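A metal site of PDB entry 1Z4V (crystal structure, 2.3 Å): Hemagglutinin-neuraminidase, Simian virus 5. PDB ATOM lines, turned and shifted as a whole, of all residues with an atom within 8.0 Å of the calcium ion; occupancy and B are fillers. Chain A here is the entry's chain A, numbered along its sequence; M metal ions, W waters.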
ATOM      1  N   GLN A 212      -2.831   4.016  -5.413  1.00  0.00           N
ATOM      2  CA  GLN A 212      -3.898   4.679  -6.147  1.00  0.00           C
ATOM      3  C   GLN A 212      -3.326   5.890  -6.890  1.00  0.00           C
ATOM      4  O   GLN A 212      -2.231   6.353  -6.577  1.00  0.00           O
ATOM      5  CB  GLN A 212      -4.957   5.143  -5.167  1.00  0.00           C
ATOM      6  CG  GLN A 212      -4.476   6.249  -4.237  1.00  0.00           C
ATOM      7  CD  GLN A 212      -5.431   6.503  -3.101  1.00  0.00           C
ATOM      8  OE1 GLN A 212      -6.643   6.345  -3.256  1.00  0.00           O
ATOM      9  NE2 GLN A 212      -4.910   6.911  -1.944  1.00  0.00           N
ATOM     10  N   GLU A 214      -2.112   9.418  -8.055  1.00  0.00           N
ATOM     11  CA  GLU A 214      -1.588  10.501  -7.241  1.00  0.00           C
ATOM     12  C   GLU A 214      -2.640  11.465  -6.742  1.00  0.00           C
ATOM     13  O   GLU A 214      -2.654  11.847  -5.568  1.00  0.00           O
ATOM     14  CB  GLU A 214      -0.509  11.280  -8.020  1.00  0.00           C
ATOM     15  CG  GLU A 214      -0.127  12.591  -7.371  1.00  0.00           C
ATOM     16  CD  GLU A 214       1.009  13.287  -8.083  1.00  0.00           C
ATOM     17  OE1 GLU A 214       0.984  13.311  -9.324  1.00  0.00           O
ATOM     18  OE2 GLU A 214       1.917  13.810  -7.396  1.00  0.00           O
ATOM     19  N   ARG A 215      -3.532  11.879  -7.638  1.00  0.00           N
ATOM     20  CA  ARG A 215      -4.569  12.831  -7.248  1.00  0.00           C
ATOM     21  C   ARG A 215      -5.424  12.294  -6.102  1.00  0.00           C
ATOM     22  O   ARG A 215      -5.818  13.035  -5.203  1.00  0.00           O
ATOM     23  CB  ARG A 215      -5.453  13.160  -8.450  1.00  0.00           C
ATOM     24  CG  ARG A 215      -6.342  14.342  -8.203  1.00  0.00           C
ATOM     25  CD  ARG A 215      -7.322  14.537  -9.332  1.00  0.00           C
ATOM     26  NE  ARG A 215      -8.259  15.613  -9.022  1.00  0.00           N
ATOM     27  CZ  ARG A 215      -9.465  15.723  -9.568  1.00  0.00           C
ATOM     28  NH1 ARG A 215      -9.872  14.821 -10.459  1.00  0.00           N
ATOM     29  NH2 ARG A 215     -10.260  16.724  -9.231  1.00  0.00           N
ATOM     30  N   ASP A 216      -5.691  10.986  -6.134  1.00  0.00           N
ATOM     31  CA  ASP A 216      -6.491  10.361  -5.079  1.00  0.00           C
ATOM     32  C   ASP A 216      -5.798  10.500  -3.730  1.00  0.00           C
ATOM     33  O   ASP A 216      -6.463  10.633  -2.698  1.00  0.00           O
ATOM     34  CB  ASP A 216      -6.729   8.882  -5.405  1.00  0.00           C
ATOM     35  CG  ASP A 216      -7.596   8.685  -6.643  1.00  0.00           C
ATOM     36  OD1 ASP A 216      -7.954   9.689  -7.296  1.00  0.00           O
ATOM     37  OD2 ASP A 216      -7.925   7.529  -6.974  1.00  0.00           O
ATOM     38  N   ASP A 217      -4.467  10.463  -3.733  1.00  0.00           N
ATOM     39  CA  ASP A 217      -3.708  10.601  -2.490  1.00  0.00           C
ATOM     40  C   ASP A 217      -4.017  11.940  -1.828  1.00  0.00           C
ATOM     41  O   ASP A 217      -4.114  12.036  -0.617  1.00  0.00           O
ATOM     42  CB  ASP A 217      -2.208  10.522  -2.729  1.00  0.00           C
ATOM     43  CG  ASP A 217      -1.719   9.111  -2.971  1.00  0.00           C
ATOM     44  OD1 ASP A 217      -2.261   8.189  -2.334  1.00  0.00           O
ATOM     45  OD2 ASP A 217      -0.796   8.926  -3.796  1.00  0.00           O
ATOM     46  N   TYR A 218      -4.177  12.995  -2.607  1.00  0.00           N
ATOM     47  CA  TYR A 218      -4.464  14.295  -2.009  1.00  0.00           C
ATOM     48  C   TYR A 218      -5.866  14.404  -1.410  1.00  0.00           C
ATOM     49  O   TYR A 218      -6.062  15.083  -0.397  1.00  0.00           O
ATOM     50  CB  TYR A 218      -4.227  15.406  -3.024  1.00  0.00           C
ATOM     51  CG  TYR A 218      -2.759  15.621  -3.334  1.00  0.00           C
ATOM     52  CD1 TYR A 218      -2.052  14.750  -4.159  1.00  0.00           C
ATOM     53  CD2 TYR A 218      -2.042  16.666  -2.718  1.00  0.00           C
ATOM     54  CE1 TYR A 218      -0.684  14.903  -4.373  1.00  0.00           C
ATOM     55  CE2 TYR A 218      -0.671  16.828  -2.930  1.00  0.00           C
ATOM     56  CZ  TYR A 218      -0.004  15.940  -3.754  1.00  0.00           C
ATOM     57  OH  TYR A 218       1.353  16.068  -3.938  1.00  0.00           O
ATOM     58  N   PHE A 219      -6.845  13.735  -2.017  1.00  0.00           N
ATOM     59  CA  PHE A 219      -8.218  13.754  -1.508  1.00  0.00           C
ATOM     60  C   PHE A 219      -8.410  12.909  -0.254  1.00  0.00           C
ATOM     61  O   PHE A 219      -9.154  13.303   0.645  1.00  0.00           O
ATOM     62  CB  PHE A 219      -9.212  13.315  -2.583  1.00  0.00           C
ATOM     63  CG  PHE A 219      -9.525  14.384  -3.579  1.00  0.00           C
ATOM     64  CD1 PHE A 219      -8.699  14.609  -4.668  1.00  0.00           C
ATOM     65  CD2 PHE A 219     -10.620  15.227  -3.377  1.00  0.00           C
ATOM     66  CE1 PHE A 219      -8.959  15.651  -5.546  1.00  0.00           C
ATOM     67  CE2 PHE A 219     -10.880  16.269  -4.255  1.00  0.00           C
ATOM     68  CZ  PHE A 219     -10.054  16.482  -5.337  1.00  0.00           C
ATOM     69  N   SER A 220      -7.783  11.745  -0.193  1.00  0.00           N
ATOM     70  CA  SER A 220      -7.906  10.911   0.995  1.00  0.00           C
ATOM     71  C   SER A 220      -7.213  11.612   2.158  1.00  0.00           C
ATOM     72  O   SER A 220      -6.121  12.157   2.003  1.00  0.00           O
ATOM     73  CB  SER A 220      -7.295   9.519   0.747  1.00  0.00           C
ATOM     74  OG  SER A 220      -5.941   9.586   0.370  1.00  0.00           O
ATOM     75  N   ALA A 221      -7.850  11.648   3.314  1.00  0.00           N
ATOM     76  CA  ALA A 221      -7.274  12.319   4.475  1.00  0.00           C
ATOM     77  C   ALA A 221      -6.120  11.511   5.077  1.00  0.00           C
ATOM     78  O   ALA A 221      -5.320  12.043   5.858  1.00  0.00           O
ATOM     79  CB  ALA A 221      -8.350  12.555   5.519  1.00  0.00           C
ATOM     80  N   ALA A 222      -6.047  10.241   4.745  1.00  0.00           N
ATOM     81  CA  ALA A 222      -4.988   9.378   5.274  1.00  0.00           C
ATOM     82  C   ALA A 222      -3.801   9.405   4.326  1.00  0.00           C
ATOM     83  O   ALA A 222      -3.971   9.256   3.130  1.00  0.00           O
ATOM     84  CB  ALA A 222      -5.500   7.946   5.419  1.00  0.00           C
ATOM     85  N   PRO A 223      -2.584   9.563   4.840  1.00  0.00           N
ATOM     86  CA  PRO A 223      -1.372   9.615   4.022  1.00  0.00           C
ATOM     87  C   PRO A 223      -0.902   8.216   3.626  1.00  0.00           C
ATOM     88  O   PRO A 223      -1.208   7.244   4.315  1.00  0.00           O
ATOM     89  CB  PRO A 223      -0.377  10.302   4.941  1.00  0.00           C
ATOM     90  CG  PRO A 223      -0.739   9.691   6.276  1.00  0.00           C
ATOM     91  CD  PRO A 223      -2.251   9.747   6.269  1.00  0.00           C
ATOM     92  N   PRO A 224      -0.160   8.106   2.516  1.00  0.00           N
ATOM     93  CA  PRO A 224       0.338   6.795   2.072  1.00  0.00           C
ATOM     94  C   PRO A 224       1.357   6.271   3.084  1.00  0.00           C
ATOM     95  O   PRO A 224       1.874   7.038   3.895  1.00  0.00           O
ATOM     96  CB  PRO A 224       0.995   7.104   0.733  1.00  0.00           C
ATOM     97  CG  PRO A 224       0.319   8.340   0.271  1.00  0.00           C
ATOM     98  CD  PRO A 224       0.187   9.143   1.534  1.00  0.00           C
ATOM     99  N   TRP A 251      -0.855  15.909   7.028  1.00  0.00           N
ATOM    100  CA  TRP A 251      -0.549  15.757   5.614  1.00  0.00           C
ATOM    101  C   TRP A 251      -1.474  14.712   4.971  1.00  0.00           C
ATOM    102  O   TRP A 251      -1.506  13.572   5.412  1.00  0.00           O
ATOM    103  CB  TRP A 251       0.898  15.290   5.424  1.00  0.00           C
ATOM    104  CG  TRP A 251       1.943  16.267   5.880  1.00  0.00           C
ATOM    105  CD1 TRP A 251       2.223  16.638   7.166  1.00  0.00           C
ATOM    106  CD2 TRP A 251       2.865  16.987   5.046  1.00  0.00           C
ATOM    107  NE1 TRP A 251       3.260  17.547   7.187  1.00  0.00           N
ATOM    108  CE2 TRP A 251       3.667  17.775   5.903  1.00  0.00           C
ATOM    109  CE3 TRP A 251       3.086  17.049   3.661  1.00  0.00           C
ATOM    110  CZ2 TRP A 251       4.686  18.618   5.411  1.00  0.00           C
ATOM    111  CZ3 TRP A 251       4.093  17.884   3.172  1.00  0.00           C
ATOM    112  CH2 TRP A 251       4.879  18.651   4.051  1.00  0.00           C
ATOM    113  N   ALA A 252      -2.204  15.106   3.936  1.00  0.00           N
ATOM    114  CA  ALA A 252      -3.060  14.155   3.251  1.00  0.00           C
ATOM    115  C   ALA A 252      -2.129  13.227   2.480  1.00  0.00           C
ATOM    116  O   ALA A 252      -2.411  12.064   2.327  1.00  0.00           O
ATOM    117  CB  ALA A 252      -4.025  14.872   2.309  1.00  0.00           C
ATOM    118  N   THR A 253      -1.012  13.752   2.003  1.00  0.00           N
ATOM    119  CA  THR A 253      -0.011  12.945   1.298  1.00  0.00           C
ATOM    120  C   THR A 253       1.360  13.444   1.656  1.00  0.00           C
ATOM    121  O   THR A 253       1.526  14.587   2.076  1.00  0.00           O
ATOM    122  CB  THR A 253      -0.069  13.051  -0.227  1.00  0.00           C
ATOM    123  OG1 THR A 253      -1.254  13.725  -0.631  1.00  0.00           O
ATOM    124  CG2 THR A 253       0.001  11.673  -0.833  1.00  0.00           C
ATOM    125  N   LEU A 254       2.346  12.580   1.440  1.00  0.00           N
ATOM    126  CA  LEU A 254       3.741  12.891   1.715  1.00  0.00           C
ATOM    127  C   LEU A 254       4.564  12.028   0.762  1.00  0.00           C
ATOM    128  O   LEU A 254       4.324  10.826   0.655  1.00  0.00           O
ATOM    129  CB  LEU A 254       4.062  12.554   3.174  1.00  0.00           C
ATOM    130  CG  LEU A 254       5.477  12.812   3.680  1.00  0.00           C
ATOM    131  CD1 LEU A 254       5.886  14.275   3.432  1.00  0.00           C
ATOM    132  CD2 LEU A 254       5.523  12.500   5.169  1.00  0.00           C
ATOM    133  N   GLY A 275       0.638  17.413   0.399  1.00  0.00           N
ATOM    134  CA  GLY A 275      -0.478  18.314   0.625  1.00  0.00           C
ATOM    135  C   GLY A 275      -0.880  18.350   2.085  1.00  0.00           C
ATOM    136  O   GLY A 275      -1.063  17.300   2.713  1.00  0.00           O
ATOM    137  N   ILE A 277      -3.517  19.486   5.169  1.00  0.00           N
ATOM    138  CA  ILE A 277      -4.944  19.657   5.411  1.00  0.00           C
ATOM    139  C   ILE A 277      -5.344  21.011   6.017  1.00  0.00           C
ATOM    140  O   ILE A 277      -4.711  21.506   6.951  1.00  0.00           O
ATOM    141  CB  ILE A 277      -5.448  18.533   6.326  1.00  0.00           C
ATOM    142  CG1 ILE A 277      -5.260  17.186   5.626  1.00  0.00           C
ATOM    143  CG2 ILE A 277      -6.913  18.759   6.720  1.00  0.00           C
ATOM    144  CD1 ILE A 277      -5.531  15.978   6.506  1.00  0.00           C
ATOM    145  N   ARG A 323      -5.593  21.028  -0.965  1.00  0.00           N
ATOM    146  CA  ARG A 323      -4.542  20.976   0.047  1.00  0.00           C
ATOM    147  C   ARG A 323      -3.520  22.074  -0.190  1.00  0.00           C
ATOM    148  O   ARG A 323      -3.423  22.621  -1.286  1.00  0.00           O
ATOM    149  CB  ARG A 323      -3.813  19.627  -0.024  1.00  0.00           C
ATOM    150  CG  ARG A 323      -4.695  18.401  -0.035  1.00  0.00           C
ATOM    151  CD  ARG A 323      -5.564  18.347   1.187  1.00  0.00           C
ATOM    152  NE  ARG A 323      -6.306  17.090   1.260  1.00  0.00           N
ATOM    153  CZ  ARG A 323      -7.267  16.849   2.133  1.00  0.00           C
ATOM    154  NH1 ARG A 323      -7.610  17.782   3.019  1.00  0.00           N
ATOM    155  NH2 ARG A 323      -7.890  15.672   2.134  1.00  0.00           N
HETATM  156 CA    CA M   1      -4.044  10.804   1.357  1.00  0.00          CA
HETATM  157  O   HOH W   1      -2.779   8.238   0.261  1.00  0.00           O
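OD1 of Asp 217 lies within hydrogen-bond range of NE2 of Gln 212 (3.0 Å). The backbone carbonyl oxygen of Asp 217 sits close to the side-chain hydroxyl of Thr 253. O of Asp 216 lies close to OG of Ser 220. O of Gly 275 is in hydrogen-bond range of N of Ala 252, 2.8 Å away.
The calcium ion is bound by O of Ala 252, 2.3 Å away. The backbone carbonyl oxygen (O) of Asp 217 binds the calcium ion (2.3 Å). The calcium ion is bound by O of Ala 222, at 2.4 Å. The calcium ion is bound by OG of Ser 220. O of Ser 220 binds the calcium ion, 2.6 Å away. Slightly farther from the calcium ion lies water W1 (3.1 Å).
Pro 223 touches the calcium ion (CA to CA, 3.96 Å). Of the 19 residues printed, 5 come within 4 Å of the calcium ion.
Water W1 lies within hydrogen-bond range of the side-chain carboxylate of Asp 217 (2.6 Å) and the side-chain amide nitrogen of Gln 212 (3.3 Å).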
